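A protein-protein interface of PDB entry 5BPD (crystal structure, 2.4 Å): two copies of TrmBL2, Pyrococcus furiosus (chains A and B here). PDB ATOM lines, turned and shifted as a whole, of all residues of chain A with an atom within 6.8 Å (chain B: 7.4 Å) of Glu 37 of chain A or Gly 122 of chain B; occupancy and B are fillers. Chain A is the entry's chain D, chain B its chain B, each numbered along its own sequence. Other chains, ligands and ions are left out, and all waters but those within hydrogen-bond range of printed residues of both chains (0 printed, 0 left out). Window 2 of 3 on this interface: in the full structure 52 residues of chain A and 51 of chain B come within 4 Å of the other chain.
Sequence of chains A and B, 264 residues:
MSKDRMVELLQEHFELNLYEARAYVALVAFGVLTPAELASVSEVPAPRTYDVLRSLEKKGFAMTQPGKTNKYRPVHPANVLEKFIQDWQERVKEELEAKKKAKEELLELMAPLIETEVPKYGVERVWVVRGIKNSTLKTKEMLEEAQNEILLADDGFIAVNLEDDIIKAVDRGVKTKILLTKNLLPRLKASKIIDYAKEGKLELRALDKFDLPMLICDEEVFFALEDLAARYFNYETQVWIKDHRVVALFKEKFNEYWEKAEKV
N of Val 123 of chain B lies within hydrogen-bond range of OE2 of Glu 37 of chain A (3.4 Å).
N of Thr 34 of chain A lies within hydrogen-bond range of OE1 of Glu 37 of chain A (2.9 Å).
Among the printed residues, merely in contact across the chains: Val 32 of chain A with Pro 119 of chain B (3.2 Å), Glu 37 of chain A with Gly 122 of chain B (3.3 Å), Phe 30 of chain A with Pro 119 of chain B (3.5 Å), Leu 33 of chain A with Val 123 of chain B (3.5 Å), Val 32 of chain A with Val 123 of chain B (3.6 Å), Lys 71 of chain A with Lys 120 of chain B (3.7 Å) and Lys 71 of chain A with Gly 122 of chain B (3.95 Å).
Glu 37 of chain A touches two residues of chain B. Ala 36 of chain A touches none of the printed residues of chain B. Of the printed residues of chain A, Pro 119 of chain B touches Phe 30 (3.5 Å) and Val 32 (3.2 Å). Of the printed residues of chain A, Val 123 of chain B touches Val 32, Leu 33 and Glu 37. Of the printed residues of chain B, Lys 71 of chain A touches Lys 120 (3.7 Å) and Gly 122 (3.95 Å). Of the printed residues of chain B, Val 32 of chain A touches Pro 119 and Val 123. Val 118 of chain B touches none of the printed residues of chain A. The nearest residue of chain A that does not touch Gly 122 of chain B is Val 32 of chain A (5.8 Å). The nearest printed residue of chain A that does not touch Val 123 of chain B is Phe 30 of chain A (4.1 Å).
Of the 14 printed residues of chain A, 5 touch a printed residue of chain B. Of the 10 printed residues of chain B, 4 touch a printed residue of chain A. Hydrophobic or aromatic side chains of chain B within 4 Å of the printed part of chain A: Pro 119 and Val 123. Among the printed residues, no Asp or Glu carboxylate lies within 4 Å of a Lys or Arg side-chain nitrogen of the other chain.
No position is printed for both chains. Of the 8 pairs that touch across the chains among the printed residues, none has its exchanged pair printed and touching as well.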
ATOM      1  N   PHE A  30     -19.259  26.882   3.817  1.00  0.00           N
ATOM      2  CA  PHE A  30     -19.036  26.033   4.986  1.00  0.00           C
ATOM      3  C   PHE A  30     -19.521  24.591   4.825  1.00  0.00           C
ATOM      4  O   PHE A  30     -19.348  23.775   5.731  1.00  0.00           O
ATOM      5  CB  PHE A  30     -19.704  26.654   6.216  1.00  0.00           C
ATOM      6  CG  PHE A  30     -19.186  28.019   6.562  1.00  0.00           C
ATOM      7  CD1 PHE A  30     -17.973  28.168   7.209  1.00  0.00           C
ATOM      8  CD2 PHE A  30     -19.911  29.152   6.235  1.00  0.00           C
ATOM      9  CE1 PHE A  30     -17.489  29.426   7.528  1.00  0.00           C
ATOM     10  CE2 PHE A  30     -19.435  30.414   6.551  1.00  0.00           C
ATOM     11  CZ  PHE A  30     -18.222  30.551   7.199  1.00  0.00           C
ATOM     12  N   VAL A  32     -21.944  22.696   5.375  1.00  0.00           N
ATOM     13  CA  VAL A  32     -23.165  22.377   6.110  1.00  0.00           C
ATOM     14  C   VAL A  32     -23.414  23.450   7.166  1.00  0.00           C
ATOM     15  O   VAL A  32     -22.477  23.943   7.789  1.00  0.00           O
ATOM     16  CB  VAL A  32     -23.089  20.983   6.760  1.00  0.00           C
ATOM     17  CG1 VAL A  32     -24.326  20.728   7.615  1.00  0.00           C
ATOM     18  CG2 VAL A  32     -22.932  19.904   5.699  1.00  0.00           C
ATOM     19  N   LEU A  33     -24.676  23.810   7.368  1.00  0.00           N
ATOM     20  CA  LEU A  33     -25.011  24.849   8.330  1.00  0.00           C
ATOM     21  C   LEU A  33     -26.343  24.600   9.024  1.00  0.00           C
ATOM     22  O   LEU A  33     -27.287  24.074   8.433  1.00  0.00           O
ATOM     23  CB  LEU A  33     -25.037  26.221   7.653  1.00  0.00           C
ATOM     24  CG  LEU A  33     -23.671  26.832   7.348  1.00  0.00           C
ATOM     25  CD1 LEU A  33     -23.828  28.244   6.812  1.00  0.00           C
ATOM     26  CD2 LEU A  33     -22.782  26.811   8.580  1.00  0.00           C
ATOM     27  N   THR A  34     -26.392  24.971  10.296  1.00  0.00           N
ATOM     28  CA  THR A  34     -27.633  25.040  11.044  1.00  0.00           C
ATOM     29  C   THR A  34     -28.202  26.445  10.862  1.00  0.00           C
ATOM     30  O   THR A  34     -27.446  27.387  10.628  1.00  0.00           O
ATOM     31  CB  THR A  34     -27.405  24.724  12.542  1.00  0.00           C
ATOM     32  OG1 THR A  34     -27.219  23.312  12.713  1.00  0.00           O
ATOM     33  CG2 THR A  34     -28.575  25.190  13.392  1.00  0.00           C
ATOM     34  N   PRO A  35     -29.533  26.589  10.937  1.00  0.00           N
ATOM     35  CA  PRO A  35     -30.130  27.926  10.883  1.00  0.00           C
ATOM     36  C   PRO A  35     -29.464  28.887  11.868  1.00  0.00           C
ATOM     37  O   PRO A  35     -29.258  30.063  11.556  1.00  0.00           O
ATOM     38  CB  PRO A  35     -31.587  27.671  11.268  1.00  0.00           C
ATOM     39  CG  PRO A  35     -31.844  26.271  10.823  1.00  0.00           C
ATOM     40  CD  PRO A  35     -30.554  25.529  11.026  1.00  0.00           C
ATOM     41  N   ALA A  36     -29.115  28.370  13.042  1.00  0.00           N
ATOM     42  CA  ALA A  36     -28.414  29.142  14.058  1.00  0.00           C
ATOM     43  C   ALA A  36     -27.015  29.517  13.587  1.00  0.00           C
ATOM     44  O   ALA A  36     -26.616  30.679  13.667  1.00  0.00           O
ATOM     45  CB  ALA A  36     -28.345  28.362  15.359  1.00  0.00           C
ATOM     46  N   GLU A  37     -26.269  28.528  13.101  1.00  0.00           N
ATOM     47  CA  GLU A  37     -24.919  28.768  12.601  1.00  0.00           C
ATOM     48  C   GLU A  37     -24.935  29.764  11.445  1.00  0.00           C
ATOM     49  O   GLU A  37     -24.011  30.562  11.292  1.00  0.00           O
ATOM     50  CB  GLU A  37     -24.265  27.459  12.151  1.00  0.00           C
ATOM     51  CG  GLU A  37     -24.035  26.452  13.266  1.00  0.00           C
ATOM     52  CD  GLU A  37     -23.492  25.124  12.761  1.00  0.00           C
ATOM     53  OE1 GLU A  37     -23.828  24.730  11.626  1.00  0.00           O
ATOM     54  OE2 GLU A  37     -22.724  24.474  13.501  1.00  0.00           O
ATOM     55  N   LEU A  38     -25.986  29.714  10.633  1.00  0.00           N
ATOM     56  CA  LEU A  38     -26.116  30.619   9.493  1.00  0.00           C
ATOM     57  C   LEU A  38     -26.260  32.067   9.950  1.00  0.00           C
ATOM     58  O   LEU A  38     -25.610  32.963   9.416  1.00  0.00           O
ATOM     59  CB  LEU A  38     -27.310  30.223   8.619  1.00  0.00           C
ATOM     60  CG  LEU A  38     -27.715  31.227   7.533  1.00  0.00           C
ATOM     61  CD1 LEU A  38     -26.576  31.457   6.555  1.00  0.00           C
ATOM     62  CD2 LEU A  38     -28.962  30.758   6.798  1.00  0.00           C
ATOM     63  N   ALA A  39     -27.120  32.291  10.938  1.00  0.00           N
ATOM     64  CA  ALA A  39     -27.350  33.631  11.465  1.00  0.00           C
ATOM     65  C   ALA A  39     -26.078  34.185  12.098  1.00  0.00           C
ATOM     66  O   ALA A  39     -25.806  35.384  12.029  1.00  0.00           O
ATOM     67  CB  ALA A  39     -28.485  33.618  12.476  1.00  0.00           C
ATOM     68  N   SER A  40     -25.308  33.292  12.711  1.00  0.00           N
ATOM     69  CA  SER A  40     -24.077  33.655  13.402  1.00  0.00           C
ATOM     70  C   SER A  40     -22.988  34.165  12.464  1.00  0.00           C
ATOM     71  O   SER A  40     -22.355  35.186  12.731  1.00  0.00           O
ATOM     72  CB  SER A  40     -23.555  32.454  14.189  1.00  0.00           C
ATOM     73  OG  SER A  40     -24.505  32.036  15.153  1.00  0.00           O
ATOM     74  N   VAL A  41     -22.771  33.445  11.370  1.00  0.00           N
ATOM     75  CA  VAL A  41     -21.672  33.739  10.461  1.00  0.00           C
ATOM     76  C   VAL A  41     -22.083  34.670   9.326  1.00  0.00           C
ATOM     77  O   VAL A  41     -21.240  35.099   8.541  1.00  0.00           O
ATOM     78  CB  VAL A  41     -21.087  32.441   9.882  1.00  0.00           C
ATOM     79  CG1 VAL A  41     -22.103  31.762   8.974  1.00  0.00           C
ATOM     80  CG2 VAL A  41     -19.798  32.726   9.129  1.00  0.00           C
ATOM     81  N   SER A  42     -23.371  34.986   9.230  1.00  0.00           N
ATOM     82  CA  SER A  42     -23.856  35.771   8.098  1.00  0.00           C
ATOM     83  C   SER A  42     -24.690  36.970   8.537  1.00  0.00           C
ATOM     84  O   SER A  42     -25.015  37.120   9.717  1.00  0.00           O
ATOM     85  CB  SER A  42     -24.675  34.892   7.145  1.00  0.00           C
ATOM     86  OG  SER A  42     -25.950  34.592   7.685  1.00  0.00           O
ATOM     87  N   THR A  49     -33.605  33.097   9.303  1.00  0.00           N
ATOM     88  CA  THR A  49     -32.787  32.007   8.780  1.00  0.00           C
ATOM     89  C   THR A  49     -33.602  30.758   8.456  1.00  0.00           C
ATOM     90  O   THR A  49     -33.309  30.050   7.493  1.00  0.00           O
ATOM     91  CB  THR A  49     -31.677  31.623   9.774  1.00  0.00           C
ATOM     92  OG1 THR A  49     -32.251  31.387  11.069  1.00  0.00           O
ATOM     93  CG2 THR A  49     -30.642  32.723   9.865  1.00  0.00           C
ATOM     94  N   LYS A  71     -30.221  20.660   9.653  1.00  0.00           N
ATOM     95  CA  LYS A  71     -28.954  20.920   8.982  1.00  0.00           C
ATOM     96  C   LYS A  71     -29.136  20.950   7.472  1.00  0.00           C
ATOM     97  O   LYS A  71     -29.748  20.057   6.890  1.00  0.00           O
ATOM     98  CB  LYS A  71     -27.910  19.869   9.364  1.00  0.00           C
ATOM     99  CG  LYS A  71     -27.346  20.028  10.767  1.00  0.00           C
ATOM    100  CD  LYS A  71     -26.067  19.227  10.925  1.00  0.00           C
ATOM    101  CE  LYS A  71     -25.413  19.487  12.268  1.00  0.00           C
ATOM    102  NZ  LYS A  71     -24.067  18.858  12.340  1.00  0.00           N
ATOM    103  N   VAL B 118     -17.353  17.690   4.724  1.00  0.00           N
ATOM    104  CA  VAL B 118     -18.612  17.975   5.396  1.00  0.00           C
ATOM    105  C   VAL B 118     -18.387  18.123   6.896  1.00  0.00           C
ATOM    106  O   VAL B 118     -17.885  17.205   7.546  1.00  0.00           O
ATOM    107  CB  VAL B 118     -19.658  16.885   5.098  1.00  0.00           C
ATOM    108  CG1 VAL B 118     -19.983  16.858   3.613  1.00  0.00           C
ATOM    109  CG2 VAL B 118     -19.159  15.525   5.562  1.00  0.00           C
ATOM    110  N   PRO B 119     -18.751  19.290   7.449  1.00  0.00           N
ATOM    111  CA  PRO B 119     -18.584  19.544   8.884  1.00  0.00           C
ATOM    112  C   PRO B 119     -19.283  18.471   9.705  1.00  0.00           C
ATOM    113  O   PRO B 119     -20.486  18.248   9.549  1.00  0.00           O
ATOM    114  CB  PRO B 119     -19.235  20.918   9.082  1.00  0.00           C
ATOM    115  CG  PRO B 119     -20.137  21.088   7.904  1.00  0.00           C
ATOM    116  CD  PRO B 119     -19.432  20.404   6.773  1.00  0.00           C
ATOM    117  N   LYS B 120     -18.526  17.812  10.571  1.00  0.00           N
ATOM    118  CA  LYS B 120     -19.029  16.658  11.300  1.00  0.00           C
ATOM    119  C   LYS B 120     -20.070  17.038  12.352  1.00  0.00           C
ATOM    120  O   LYS B 120     -21.207  16.562  12.314  1.00  0.00           O
ATOM    121  CB  LYS B 120     -17.862  15.921  11.955  1.00  0.00           C
ATOM    122  CG  LYS B 120     -16.841  15.387  10.959  1.00  0.00           C
ATOM    123  CD  LYS B 120     -17.436  14.312  10.060  1.00  0.00           C
ATOM    124  CE  LYS B 120     -16.551  14.060   8.846  1.00  0.00           C
ATOM    125  NZ  LYS B 120     -17.267  13.309   7.778  1.00  0.00           N
ATOM    126  N   TYR B 121     -19.683  17.905  13.281  1.00  0.00           N
ATOM    127  CA  TYR B 121     -20.566  18.316  14.367  1.00  0.00           C
ATOM    128  C   TYR B 121     -20.668  19.833  14.448  1.00  0.00           C
ATOM    129  O   TYR B 121     -20.812  20.400  15.532  1.00  0.00           O
ATOM    130  CB  TYR B 121     -20.085  17.742  15.703  1.00  0.00           C
ATOM    131  CG  TYR B 121     -20.142  16.232  15.772  1.00  0.00           C
ATOM    132  CD1 TYR B 121     -21.361  15.563  15.765  1.00  0.00           C
ATOM    133  CD2 TYR B 121     -18.982  15.476  15.853  1.00  0.00           C
ATOM    134  CE1 TYR B 121     -21.420  14.183  15.826  1.00  0.00           C
ATOM    135  CE2 TYR B 121     -19.032  14.096  15.920  1.00  0.00           C
ATOM    136  CZ  TYR B 121     -20.252  13.454  15.904  1.00  0.00           C
ATOM    137  OH  TYR B 121     -20.304  12.081  15.968  1.00  0.00           O
ATOM    138  N   GLY B 122     -20.595  20.488  13.294  1.00  0.00           N
ATOM    139  CA  GLY B 122     -20.714  21.932  13.230  1.00  0.00           C
ATOM    140  C   GLY B 122     -19.507  22.591  12.594  1.00  0.00           C
ATOM    141  O   GLY B 122     -18.573  21.917  12.161  1.00  0.00           O
ATOM    142  N   VAL B 123     -19.522  23.918  12.545  1.00  0.00           N
ATOM    143  CA  VAL B 123     -18.441  24.670  11.921  1.00  0.00           C
ATOM    144  C   VAL B 123     -17.466  25.209  12.959  1.00  0.00           C
ATOM    145  O   VAL B 123     -16.395  25.703  12.614  1.00  0.00           O
ATOM    146  CB  VAL B 123     -19.002  25.809  11.068  1.00  0.00           C
ATOM    147  CG1 VAL B 123     -19.943  25.253  10.012  1.00  0.00           C
ATOM    148  CG2 VAL B 123     -19.723  26.814  11.949  1.00  0.00           C
ATOM    149  N   GLU B 124     -17.845  25.116  14.231  1.00  0.00           N
ATOM    150  CA  GLU B 124     -16.990  25.578  15.318  1.00  0.00           C
ATOM    151  C   GLU B 124     -15.653  24.841  15.312  1.00  0.00           C
ATOM    152  O   GLU B 124     -15.604  23.628  15.137  1.00  0.00           O
ATOM    153  CB  GLU B 124     -17.685  25.393  16.666  1.00  0.00           C
ATOM    154  CG  GLU B 124     -17.087  26.236  17.768  1.00  0.00           C
ATOM    155  CD  GLU B 124     -17.168  27.719  17.461  1.00  0.00           C
ATOM    156  OE1 GLU B 124     -16.136  28.304  17.062  1.00  0.00           O
ATOM    157  OE2 GLU B 124     -18.265  28.294  17.615  1.00  0.00           O
ATOM    158  N   ARG B 125     -14.569  25.583  15.498  1.00  0.00           N
ATOM    159  CA  ARG B 125     -13.238  24.994  15.508  1.00  0.00           C
ATOM    160  C   ARG B 125     -12.580  25.190  16.871  1.00  0.00           C
ATOM    161  O   ARG B 125     -11.404  24.884  17.066  1.00  0.00           O
ATOM    162  CB  ARG B 125     -12.381  25.598  14.394  1.00  0.00           C
ATOM    163  CG  ARG B 125     -12.864  25.229  12.999  1.00  0.00           C
ATOM    164  CD  ARG B 125     -12.170  26.044  11.930  1.00  0.00           C
ATOM    165  NE  ARG B 125     -12.718  27.392  11.834  1.00  0.00           N
ATOM    166  CZ  ARG B 125     -11.982  28.481  11.646  1.00  0.00           C
ATOM    167  NH1 ARG B 125     -10.667  28.380  11.535  1.00  0.00           N
ATOM    168  NH2 ARG B 125     -12.561  29.670  11.574  1.00  0.00           N
ATOM    169  N   TRP B 240     -10.734  22.377  23.198  1.00  0.00           N
ATOM    170  CA  TRP B 240     -10.632  21.632  21.951  1.00  0.00           C
ATOM    171  C   TRP B 240     -10.385  22.611  20.804  1.00  0.00           C
ATOM    172  O   TRP B 240     -11.092  23.607  20.674  1.00  0.00           O
ATOM    173  CB  TRP B 240     -11.912  20.823  21.719  1.00  0.00           C
ATOM    174  CG  TRP B 240     -12.025  20.181  20.370  1.00  0.00           C
ATOM    175  CD1 TRP B 240     -11.560  18.951  20.003  1.00  0.00           C
ATOM    176  CD2 TRP B 240     -12.664  20.729  19.210  1.00  0.00           C
ATOM    177  NE1 TRP B 240     -11.866  18.702  18.688  1.00  0.00           N
ATOM    178  CE2 TRP B 240     -12.544  19.777  18.178  1.00  0.00           C
ATOM    179  CE3 TRP B 240     -13.325  21.932  18.944  1.00  0.00           C
ATOM    180  CZ2 TRP B 240     -13.055  19.993  16.900  1.00  0.00           C
ATOM    181  CZ3 TRP B 240     -13.833  22.145  17.674  1.00  0.00           C
ATOM    182  CH2 TRP B 240     -13.696  21.180  16.669  1.00  0.00           C
ATOM    183  N   LYS B 242      -9.473  22.949  16.497  1.00  0.00           N
ATOM    184  CA  LYS B 242      -9.362  22.319  15.190  1.00  0.00           C
ATOM    185  C   LYS B 242      -8.591  23.221  14.236  1.00  0.00           C
ATOM    186  O   LYS B 242      -9.161  24.108  13.603  1.00  0.00           O
ATOM    187  CB  LYS B 242     -10.750  22.002  14.624  1.00  0.00           C
ATOM    188  CG  LYS B 242     -10.733  21.088  13.412  1.00  0.00           C
ATOM    189  CD  LYS B 242     -12.145  20.723  12.992  1.00  0.00           C
ATOM    190  CE  LYS B 242     -12.151  19.617  11.948  1.00  0.00           C
ATOM    191  NZ  LYS B 242     -13.531  19.316  11.470  1.00  0.00           N
